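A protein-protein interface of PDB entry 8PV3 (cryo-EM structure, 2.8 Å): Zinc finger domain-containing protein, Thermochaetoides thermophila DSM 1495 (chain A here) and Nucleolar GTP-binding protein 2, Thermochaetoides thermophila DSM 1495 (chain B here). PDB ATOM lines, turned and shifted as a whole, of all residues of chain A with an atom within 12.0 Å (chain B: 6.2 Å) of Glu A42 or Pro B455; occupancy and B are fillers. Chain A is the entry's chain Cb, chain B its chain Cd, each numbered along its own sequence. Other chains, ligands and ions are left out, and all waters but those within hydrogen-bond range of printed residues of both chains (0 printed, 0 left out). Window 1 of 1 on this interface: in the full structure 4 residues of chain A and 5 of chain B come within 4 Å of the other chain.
Of the printed residues of chain B, Glu A42 touches Glu B440 (3.5 Å) and Pro B455 (3.997 Å).
Of the printed residues of chain A, Pro B455 touches Glu A42 (3.997 Å).
Of chain A, only Glu A42 comes within 4 Å of Glu B440.
No residue of chain A comes within 4 Å of Leu B450.
Glu B454 touches just one residue of chain A: Asp A43.
No residue of chain A comes within 4 Å of Asp B456.
Printed residues of chain B within 4 Å of Asp A43: Glu B454 (3.0 Å).
Of the printed residues of chain A, Arg B444 touches Leu A47 (3.4 Å).
Of the printed residues of chain B, Leu A47 touches Arg B444 (3.4 Å).
Gly A48 touches none of the printed residues of chain B.
Thr A38 touches none of the printed residues of chain B.
The nearest printed residue of chain B that does not touch Glu A42 is Glu B454 (5.3 Å).
The nearest printed residue of chain A that does not touch Pro B455 is Asp A43 (4.6 Å).
The nearest printed residue of chain B that does not touch Asp A43 is Pro B455 (4.6 Å).
Glu A42 touches Glu B440 (CB to OE2, 3.5 Å).
Pro B455 touches Glu A42 (CD to O, 3.997 Å).
Arg B444 touches Leu A47 (NH1 to CD2, 3.4 Å).
The side-chain carboxylate of Asp A43 lies close to the side-chain carboxylate of Glu B454 (3.0 Å).
Hydrophobic or aromatic side chains of chain B that line the printed part of chain A: Pro B455.
Hydrophobic or aromatic side chains of chain A within 4 Å of the printed part of chain B: Leu A47.
Along chain A the printed residues that touch a printed residue of chain B span positions 42 to 47.
Among the printed residues, no Asp or Glu carboxylate lies within 4 Å of a Lys or Arg side-chain nitrogen of the other chain.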
ATOM      1  N   TYR A  35       3.666  24.447   6.912  1.00  0.00           N
ATOM      2  CA  TYR A  35       3.413  23.623   5.734  1.00  0.00           C
ATOM      3  C   TYR A  35       2.726  22.316   6.120  1.00  0.00           C
ATOM      4  O   TYR A  35       2.007  21.716   5.311  1.00  0.00           O
ATOM      5  CB  TYR A  35       4.720  23.356   4.988  1.00  0.00           C
ATOM      6  CG  TYR A  35       4.565  22.465   3.776  1.00  0.00           C
ATOM      7  CD1 TYR A  35       3.700  22.810   2.744  1.00  0.00           C
ATOM      8  CD2 TYR A  35       5.278  21.280   3.666  1.00  0.00           C
ATOM      9  CE1 TYR A  35       3.555  22.001   1.635  1.00  0.00           C
ATOM     10  CE2 TYR A  35       5.138  20.464   2.561  1.00  0.00           C
ATOM     11  CZ  TYR A  35       4.276  20.829   1.549  1.00  0.00           C
ATOM     12  OH  TYR A  35       4.135  20.018   0.448  1.00  0.00           O
ATOM     13  N   LYS A  36       2.929  21.860   7.360  1.00  0.00           N
ATOM     14  CA  LYS A  36       2.202  20.678   7.810  1.00  0.00           C
ATOM     15  C   LYS A  36       0.717  20.956   8.062  1.00  0.00           C
ATOM     16  O   LYS A  36      -0.115  20.135   7.656  1.00  0.00           O
ATOM     17  CB  LYS A  36       2.853  20.060   9.051  1.00  0.00           C
ATOM     18  CG  LYS A  36       4.248  19.502   8.798  1.00  0.00           C
ATOM     19  CD  LYS A  36       4.209  18.258   7.922  1.00  0.00           C
ATOM     20  CE  LYS A  36       5.606  17.709   7.676  1.00  0.00           C
ATOM     21  NZ  LYS A  36       6.218  17.153   8.909  1.00  0.00           N
ATOM     22  N   GLU A  37       0.332  22.070   8.717  1.00  0.00           N
ATOM     23  CA  GLU A  37      -1.125  22.226   8.876  1.00  0.00           C
ATOM     24  C   GLU A  37      -1.776  22.730   7.592  1.00  0.00           C
ATOM     25  O   GLU A  37      -3.008  22.747   7.499  1.00  0.00           O
ATOM     26  CB  GLU A  37      -1.653  23.129  10.022  1.00  0.00           C
ATOM     27  CG  GLU A  37      -1.488  24.662  10.002  1.00  0.00           C
ATOM     28  CD  GLU A  37      -0.209  25.176  10.569  1.00  0.00           C
ATOM     29  OE1 GLU A  37       0.703  24.385  10.742  1.00  0.00           O
ATOM     30  OE2 GLU A  37      -0.116  26.390  10.840  1.00  0.00           O
ATOM     31  N   THR A  38      -0.990  23.138   6.591  1.00  0.00           N
ATOM     32  CA  THR A  38      -1.612  23.380   5.288  1.00  0.00           C
ATOM     33  C   THR A  38      -1.978  22.092   4.543  1.00  0.00           C
ATOM     34  O   THR A  38      -2.472  22.173   3.413  1.00  0.00           O
ATOM     35  CB  THR A  38      -0.718  24.243   4.389  1.00  0.00           C
ATOM     36  OG1 THR A  38       0.526  23.575   4.148  1.00  0.00           O
ATOM     37  CG2 THR A  38      -0.489  25.621   4.993  1.00  0.00           C
ATOM     38  N   LYS A  39      -1.756  20.921   5.135  1.00  0.00           N
ATOM     39  CA  LYS A  39      -2.193  19.651   4.578  1.00  0.00           C
ATOM     40  C   LYS A  39      -3.007  18.887   5.616  1.00  0.00           C
ATOM     41  O   LYS A  39      -2.973  19.190   6.811  1.00  0.00           O
ATOM     42  CB  LYS A  39      -1.003  18.799   4.116  1.00  0.00           C
ATOM     43  CG  LYS A  39      -0.167  19.436   3.017  1.00  0.00           C
ATOM     44  CD  LYS A  39      -0.986  19.661   1.756  1.00  0.00           C
ATOM     45  CE  LYS A  39      -1.397  18.344   1.117  1.00  0.00           C
ATOM     46  NZ  LYS A  39      -0.226  17.565   0.628  1.00  0.00           N
ATOM     47  N   ALA A  40      -3.744  17.887   5.142  1.00  0.00           N
ATOM     48  CA  ALA A  40      -4.574  17.036   5.988  1.00  0.00           C
ATOM     49  C   ALA A  40      -3.819  15.743   6.262  1.00  0.00           C
ATOM     50  O   ALA A  40      -3.369  15.078   5.325  1.00  0.00           O
ATOM     51  CB  ALA A  40      -5.921  16.747   5.327  1.00  0.00           C
ATOM     52  N   ALA A  41      -3.700  15.387   7.544  1.00  0.00           N
ATOM     53  CA  ALA A  41      -2.816  14.294   7.941  1.00  0.00           C
ATOM     54  C   ALA A  41      -3.343  12.938   7.488  1.00  0.00           C
ATOM     55  O   ALA A  41      -2.559  12.024   7.205  1.00  0.00           O
ATOM     56  CB  ALA A  41      -2.616  14.309   9.456  1.00  0.00           C
ATOM     57  N   GLU A  42      -4.667  12.780   7.423  1.00  0.00           N
ATOM     58  CA  GLU A  42      -5.238  11.481   7.085  1.00  0.00           C
ATOM     59  C   GLU A  42      -5.083  11.132   5.609  1.00  0.00           C
ATOM     60  O   GLU A  42      -5.164   9.951   5.258  1.00  0.00           O
ATOM     61  CB  GLU A  42      -6.716  11.435   7.479  1.00  0.00           C
ATOM     62  CG  GLU A  42      -7.614  12.372   6.686  1.00  0.00           C
ATOM     63  CD  GLU A  42      -7.768  13.733   7.340  1.00  0.00           C
ATOM     64  OE1 GLU A  42      -6.968  14.059   8.242  1.00  0.00           O
ATOM     65  OE2 GLU A  42      -8.694  14.475   6.952  1.00  0.00           O
ATOM     66  N   ASP A  43      -4.863  12.118   4.742  1.00  0.00           N
ATOM     67  CA  ASP A  43      -4.718  11.868   3.314  1.00  0.00           C
ATOM     68  C   ASP A  43      -3.266  11.829   2.854  1.00  0.00           C
ATOM     69  O   ASP A  43      -3.017  11.661   1.656  1.00  0.00           O
ATOM     70  CB  ASP A  43      -5.480  12.925   2.513  1.00  0.00           C
ATOM     71  CG  ASP A  43      -6.979  12.720   2.563  1.00  0.00           C
ATOM     72  OD1 ASP A  43      -7.422  11.705   3.140  1.00  0.00           O
ATOM     73  OD2 ASP A  43      -7.713  13.567   2.017  1.00  0.00           O
ATOM     74  N   LEU A  44      -2.321  11.976   3.753  1.00  0.00           N
ATOM     75  CA  LEU A  44      -0.919  11.912   3.386  1.00  0.00           C
ATOM     76  C   LEU A  44      -0.458  10.464   3.277  1.00  0.00           C
ATOM     77  O   LEU A  44      -1.030   9.577   3.918  1.00  0.00           O
ATOM     78  CB  LEU A  44      -0.061  12.647   4.421  1.00  0.00           C
ATOM     79  CG  LEU A  44      -0.344  14.144   4.562  1.00  0.00           C
ATOM     80  CD1 LEU A  44       0.649  14.808   5.495  1.00  0.00           C
ATOM     81  CD2 LEU A  44      -0.336  14.823   3.201  1.00  0.00           C
ATOM     82  N   PRO A  45       0.553  10.190   2.452  1.00  0.00           N
ATOM     83  CA  PRO A  45       1.137   8.844   2.425  1.00  0.00           C
ATOM     84  C   PRO A  45       1.804   8.510   3.753  1.00  0.00           C
ATOM     85  O   PRO A  45       2.646   9.258   4.253  1.00  0.00           O
ATOM     86  CB  PRO A  45       2.160   8.921   1.287  1.00  0.00           C
ATOM     87  CG  PRO A  45       1.733  10.067   0.452  1.00  0.00           C
ATOM     88  CD  PRO A  45       1.065  11.041   1.365  1.00  0.00           C
ATOM     89  N   GLY A  46       1.416   7.371   4.324  1.00  0.00           N
ATOM     90  CA  GLY A  46       1.938   6.980   5.619  1.00  0.00           C
ATOM     91  C   GLY A  46       1.455   7.833   6.767  1.00  0.00           C
ATOM     92  O   GLY A  46       2.140   7.918   7.791  1.00  0.00           O
ATOM     93  N   LEU A  47       0.296   8.481   6.612  1.00  0.00           N
ATOM     94  CA  LEU A  47      -0.334   9.348   7.613  1.00  0.00           C
ATOM     95  C   LEU A  47       0.555  10.519   8.027  1.00  0.00           C
ATOM     96  O   LEU A  47       0.418  11.043   9.136  1.00  0.00           O
ATOM     97  CB  LEU A  47      -0.776   8.553   8.849  1.00  0.00           C
ATOM     98  CG  LEU A  47      -1.597   7.292   8.577  1.00  0.00           C
ATOM     99  CD1 LEU A  47      -1.473   6.306   9.726  1.00  0.00           C
ATOM    100  CD2 LEU A  47      -3.054   7.647   8.326  1.00  0.00           C
ATOM    101  N   GLY A  48       1.467  10.945   7.155  1.00  0.00           N
ATOM    102  CA  GLY A  48       2.321  12.080   7.426  1.00  0.00           C
ATOM    103  C   GLY A  48       3.497  11.809   8.338  1.00  0.00           C
ATOM    104  O   GLY A  48       4.257  12.741   8.629  1.00  0.00           O
ATOM    105  N   LEU A  49       3.677  10.570   8.796  1.00  0.00           N
ATOM    106  CA  LEU A  49       4.780  10.248   9.690  1.00  0.00           C
ATOM    107  C   LEU A  49       6.121  10.181   8.975  1.00  0.00           C
ATOM    108  O   LEU A  49       7.147  10.518   9.576  1.00  0.00           O
ATOM    109  CB  LEU A  49       4.514   8.918  10.395  1.00  0.00           C
ATOM    110  CG  LEU A  49       3.331   8.886  11.364  1.00  0.00           C
ATOM    111  CD1 LEU A  49       3.101   7.474  11.881  1.00  0.00           C
ATOM    112  CD2 LEU A  49       3.552   9.855  12.514  1.00  0.00           C
ATOM    113  N   TYR A  50       6.137   9.759   7.714  1.00  0.00           N
ATOM    114  CA  TYR A  50       7.366   9.529   6.957  1.00  0.00           C
ATOM    115  C   TYR A  50       7.460  10.627   5.903  1.00  0.00           C
ATOM    116  O   TYR A  50       6.840  10.542   4.840  1.00  0.00           O
ATOM    117  CB  TYR A  50       7.371   8.133   6.337  1.00  0.00           C
ATOM    118  CG  TYR A  50       6.791   7.072   7.245  1.00  0.00           C
ATOM    119  CD1 TYR A  50       5.468   6.662   7.112  1.00  0.00           C
ATOM    120  CD2 TYR A  50       7.555   6.500   8.253  1.00  0.00           C
ATOM    121  CE1 TYR A  50       4.930   5.700   7.947  1.00  0.00           C
ATOM    122  CE2 TYR A  50       7.026   5.538   9.092  1.00  0.00           C
ATOM    123  CZ  TYR A  50       5.714   5.142   8.934  1.00  0.00           C
ATOM    124  OH  TYR A  50       5.184   4.185   9.768  1.00  0.00           O
ATOM    125  N   TRP A  58       6.243  13.074   0.986  1.00  0.00           N
ATOM    126  CA  TRP A  58       5.774  12.077   1.935  1.00  0.00           C
ATOM    127  C   TRP A  58       5.868  10.688   1.319  1.00  0.00           C
ATOM    128  O   TRP A  58       5.738  10.518   0.105  1.00  0.00           O
ATOM    129  CB  TRP A  58       4.334  12.353   2.366  1.00  0.00           C
ATOM    130  CG  TRP A  58       4.196  13.470   3.344  1.00  0.00           C
ATOM    131  CD1 TRP A  58       4.353  13.399   4.695  1.00  0.00           C
ATOM    132  CD2 TRP A  58       3.857  14.830   3.051  1.00  0.00           C
ATOM    133  NE1 TRP A  58       4.141  14.632   5.262  1.00  0.00           N
ATOM    134  CE2 TRP A  58       3.834  15.528   4.272  1.00  0.00           C
ATOM    135  CE3 TRP A  58       3.575  15.525   1.872  1.00  0.00           C
ATOM    136  CZ2 TRP A  58       3.540  16.885   4.350  1.00  0.00           C
ATOM    137  CZ3 TRP A  58       3.284  16.872   1.950  1.00  0.00           C
ATOM    138  CH2 TRP A  58       3.267  17.538   3.180  1.00  0.00           C
ATOM    139  N   PHE A  59       6.097   9.690   2.170  1.00  0.00           N
ATOM    140  CA  PHE A  59       6.283   8.321   1.721  1.00  0.00           C
ATOM    141  C   PHE A  59       5.436   7.378   2.561  1.00  0.00           C
ATOM    142  O   PHE A  59       5.056   7.687   3.693  1.00  0.00           O
ATOM    143  CB  PHE A  59       7.756   7.901   1.780  1.00  0.00           C
ATOM    144  CG  PHE A  59       8.637   8.682   0.854  1.00  0.00           C
ATOM    145  CD1 PHE A  59       9.188   9.888   1.252  1.00  0.00           C
ATOM    146  CD2 PHE A  59       8.894   8.221  -0.424  1.00  0.00           C
ATOM    147  CE1 PHE A  59       9.987  10.611   0.398  1.00  0.00           C
ATOM    148  CE2 PHE A  59       9.694   8.941  -1.283  1.00  0.00           C
ATOM    149  CZ  PHE A  59      10.236  10.138  -0.873  1.00  0.00           C
ATOM    150  N   GLU A  60       5.144   6.214   1.984  1.00  0.00           N
ATOM    151  CA  GLU A  60       4.263   5.257   2.636  1.00  0.00           C
ATOM    152  C   GLU A  60       4.955   4.477   3.745  1.00  0.00           C
ATOM    153  O   GLU A  60       4.272   3.981   4.646  1.00  0.00           O
ATOM    154  CB  GLU A  60       3.688   4.290   1.601  1.00  0.00           C
ATOM    155  CG  GLU A  60       4.738   3.568   0.776  1.00  0.00           C
ATOM    156  CD  GLU A  60       4.144   2.493  -0.110  1.00  0.00           C
ATOM    157  OE1 GLU A  60       3.040   2.707  -0.651  1.00  0.00           O
ATOM    158  OE2 GLU A  60       4.785   1.432  -0.265  1.00  0.00           O
ATOM    159  N   LEU B 439     -13.672   3.172   8.092  1.00  0.00           N
ATOM    160  CA  LEU B 439     -13.545   3.145   6.641  1.00  0.00           C
ATOM    161  C   LEU B 439     -12.094   3.306   6.206  1.00  0.00           C
ATOM    162  O   LEU B 439     -11.672   2.699   5.218  1.00  0.00           O
ATOM    163  CB  LEU B 439     -14.426   4.228   6.017  1.00  0.00           C
ATOM    164  CG  LEU B 439     -15.937   4.061   6.216  1.00  0.00           C
ATOM    165  CD1 LEU B 439     -16.705   5.242   5.652  1.00  0.00           C
ATOM    166  CD2 LEU B 439     -16.441   2.768   5.610  1.00  0.00           C
ATOM    167  N   GLU B 440     -11.307   4.095   6.946  1.00  0.00           N
ATOM    168  CA  GLU B 440      -9.892   4.251   6.609  1.00  0.00           C
ATOM    169  C   GLU B 440      -9.120   2.947   6.789  1.00  0.00           C
ATOM    170  O   GLU B 440      -8.345   2.553   5.909  1.00  0.00           O
ATOM    171  CB  GLU B 440      -9.266   5.363   7.447  1.00  0.00           C
ATOM    172  CG  GLU B 440      -9.630   6.761   6.994  1.00  0.00           C
ATOM    173  CD  GLU B 440      -9.132   7.825   7.949  1.00  0.00           C
ATOM    174  OE1 GLU B 440      -8.569   7.461   9.002  1.00  0.00           O
ATOM    175  OE2 GLU B 440      -9.304   9.025   7.649  1.00  0.00           O
ATOM    176  N   ALA B 443     -10.149   0.527   4.081  1.00  0.00           N
ATOM    177  CA  ALA B 443      -9.534   0.868   2.802  1.00  0.00           C
ATOM    178  C   ALA B 443      -8.066   0.471   2.763  1.00  0.00           C
ATOM    179  O   ALA B 443      -7.586  -0.055   1.753  1.00  0.00           O
ATOM    180  CB  ALA B 443      -9.688   2.360   2.530  1.00  0.00           C
ATOM    181  N   ARG B 444      -7.335   0.714   3.853  1.00  0.00           N
ATOM    182  CA  ARG B 444      -5.923   0.343   3.886  1.00  0.00           C
ATOM    183  C   ARG B 444      -5.742  -1.171   3.903  1.00  0.00           C
ATOM    184  O   ARG B 444      -4.775  -1.688   3.332  1.00  0.00           O
ATOM    185  CB  ARG B 444      -5.235   0.983   5.089  1.00  0.00           C
ATOM    186  CG  ARG B 444      -5.224   2.500   5.050  1.00  0.00           C
ATOM    187  CD  ARG B 444      -4.259   3.075   6.065  1.00  0.00           C
ATOM    188  NE  ARG B 444      -4.746   2.899   7.426  1.00  0.00           N
ATOM    189  CZ  ARG B 444      -5.218   3.877   8.186  1.00  0.00           C
ATOM    190  NH1 ARG B 444      -5.292   5.120   7.742  1.00  0.00           N
ATOM    191  NH2 ARG B 444      -5.628   3.600   9.421  1.00  0.00           N
ATOM    192  N   ARG B 448      -7.991  -0.412  -1.102  1.00  0.00           N
ATOM    193  CA  ARG B 448      -8.760   0.629  -1.782  1.00  0.00           C
ATOM    194  C   ARG B 448      -8.065   1.966  -1.557  1.00  0.00           C
ATOM    195  O   ARG B 448      -8.374   2.725  -0.636  1.00  0.00           O
ATOM    196  CB  ARG B 448     -10.200   0.649  -1.285  1.00  0.00           C
ATOM    197  CG  ARG B 448     -11.065  -0.490  -1.796  1.00  0.00           C
ATOM    198  CD  ARG B 448     -11.121  -0.479  -3.310  1.00  0.00           C
ATOM    199  NE  ARG B 448     -10.243  -1.485  -3.892  1.00  0.00           N
ATOM    200  CZ  ARG B 448      -9.567  -1.319  -5.018  1.00  0.00           C
ATOM    201  NH1 ARG B 448      -9.626  -0.187  -5.697  1.00  0.00           N
ATOM    202  NH2 ARG B 448      -8.805  -2.308  -5.469  1.00  0.00           N
ATOM    203  N   LEU B 449      -7.100   2.255  -2.424  1.00  0.00           N
ATOM    204  CA  LEU B 449      -6.270   3.440  -2.306  1.00  0.00           C
ATOM    205  C   LEU B 449      -6.349   4.273  -3.577  1.00  0.00           C
ATOM    206  O   LEU B 449      -6.418   3.738  -4.687  1.00  0.00           O
ATOM    207  CB  LEU B 449      -4.810   3.073  -2.027  1.00  0.00           C
ATOM    208  CG  LEU B 449      -4.556   2.081  -0.892  1.00  0.00           C
ATOM    209  CD1 LEU B 449      -3.123   1.591  -0.927  1.00  0.00           C
ATOM    210  CD2 LEU B 449      -4.880   2.718   0.448  1.00  0.00           C
ATOM    211  N   LEU B 450      -6.342   5.588  -3.399  1.00  0.00           N
ATOM    212  CA  LEU B 450      -6.276   6.522  -4.511  1.00  0.00           C
ATOM    213  C   LEU B 450      -4.810   6.834  -4.805  1.00  0.00           C
ATOM    214  O   LEU B 450      -3.904   6.136  -4.342  1.00  0.00           O
ATOM    215  CB  LEU B 450      -7.092   7.774  -4.199  1.00  0.00           C
ATOM    216  CG  LEU B 450      -8.584   7.540  -3.953  1.00  0.00           C
ATOM    217  CD1 LEU B 450      -9.291   8.844  -3.629  1.00  0.00           C
ATOM    218  CD2 LEU B 450      -9.222   6.864  -5.152  1.00  0.00           C
ATOM    219  N   GLY B 453      -1.556   6.601  -2.168  1.00  0.00           N
ATOM    220  CA  GLY B 453      -1.907   5.802  -1.013  1.00  0.00           C
ATOM    221  C   GLY B 453      -3.014   6.371  -0.159  1.00  0.00           C
ATOM    222  O   GLY B 453      -3.252   5.857   0.940  1.00  0.00           O
ATOM    223  N   GLU B 454      -3.686   7.418  -0.620  1.00  0.00           N
ATOM    224  CA  GLU B 454      -4.808   7.985   0.115  1.00  0.00           C
ATOM    225  C   GLU B 454      -5.987   7.018   0.069  1.00  0.00           C
ATOM    226  O   GLU B 454      -6.290   6.478  -1.000  1.00  0.00           O
ATOM    227  CB  GLU B 454      -5.184   9.337  -0.484  1.00  0.00           C
ATOM    228  CG  GLU B 454      -6.408   9.992   0.119  1.00  0.00           C
ATOM    229  CD  GLU B 454      -6.934  11.124  -0.736  1.00  0.00           C
ATOM    230  OE1 GLU B 454      -6.365  11.362  -1.821  1.00  0.00           O
ATOM    231  OE2 GLU B 454      -7.917  11.775  -0.327  1.00  0.00           O
ATOM    232  N   PRO B 455      -6.652   6.758   1.195  1.00  0.00           N
ATOM    233  CA  PRO B 455      -7.713   5.739   1.218  1.00  0.00           C
ATOM    234  C   PRO B 455      -8.929   6.135   0.388  1.00  0.00           C
ATOM    235  O   PRO B 455      -9.284   7.312   0.291  1.00  0.00           O
ATOM    236  CB  PRO B 455      -8.058   5.629   2.707  1.00  0.00           C
ATOM    237  CG  PRO B 455      -7.586   6.904   3.307  1.00  0.00           C
ATOM    238  CD  PRO B 455      -6.361   7.274   2.542  1.00  0.00           C
ATOM    239  N   ASP B 456      -9.570   5.127  -0.209  1.00  0.00           N
ATOM    240  CA  ASP B 456     -10.787   5.316  -1.002  1.00  0.00           C
ATOM    241  C   ASP B 456     -11.988   5.120  -0.080  1.00  0.00           C
ATOM    242  O   ASP B 456     -12.696   4.109  -0.123  1.00  0.00           O
ATOM    243  CB  ASP B 456     -10.813   4.351  -2.180  1.00  0.00           C
ATOM    244  CG  ASP B 456     -11.933   4.647  -3.158  1.00  0.00           C
ATOM    245  OD1 ASP B 456     -12.579   5.708  -3.032  1.00  0.00           O
ATOM    246  OD2 ASP B 456     -12.170   3.813  -4.057  1.00  0.00           O
ATOM    247  N   VAL B 457     -12.214   6.128   0.766  1.00  0.00           N
ATOM    248  CA  VAL B 457     -13.249   6.048   1.792  1.00  0.00           C
ATOM    249  C   VAL B 457     -14.636   6.018   1.156  1.00  0.00           C
ATOM    250  O   VAL B 457     -15.532   5.307   1.623  1.00  0.00           O
ATOM    251  CB  VAL B 457     -13.081   7.217   2.782  1.00  0.00           C
ATOM    252  CG1 VAL B 457     -14.214   7.268   3.785  1.00  0.00           C
ATOM    253  CG2 VAL B 457     -11.748   7.106   3.501  1.00  0.00           C
ATOM    254  N   ASP B 458     -14.818   6.752   0.054  1.00  0.00           N
ATOM    255  CA  ASP B 458     -16.092   6.751  -0.662  1.00  0.00           C
ATOM    256  C   ASP B 458     -16.420   5.372  -1.227  1.00  0.00           C
ATOM    257  O   ASP B 458     -17.537   4.868  -1.049  1.00  0.00           O
ATOM    258  CB  ASP B 458     -16.042   7.796  -1.778  1.00  0.00           C
ATOM    259  CG  ASP B 458     -17.415   8.181  -2.296  1.00  0.00           C
ATOM    260  OD1 ASP B 458     -18.105   7.324  -2.887  1.00  0.00           O
ATOM    261  OD2 ASP B 458     -17.797   9.357  -2.121  1.00  0.00           O
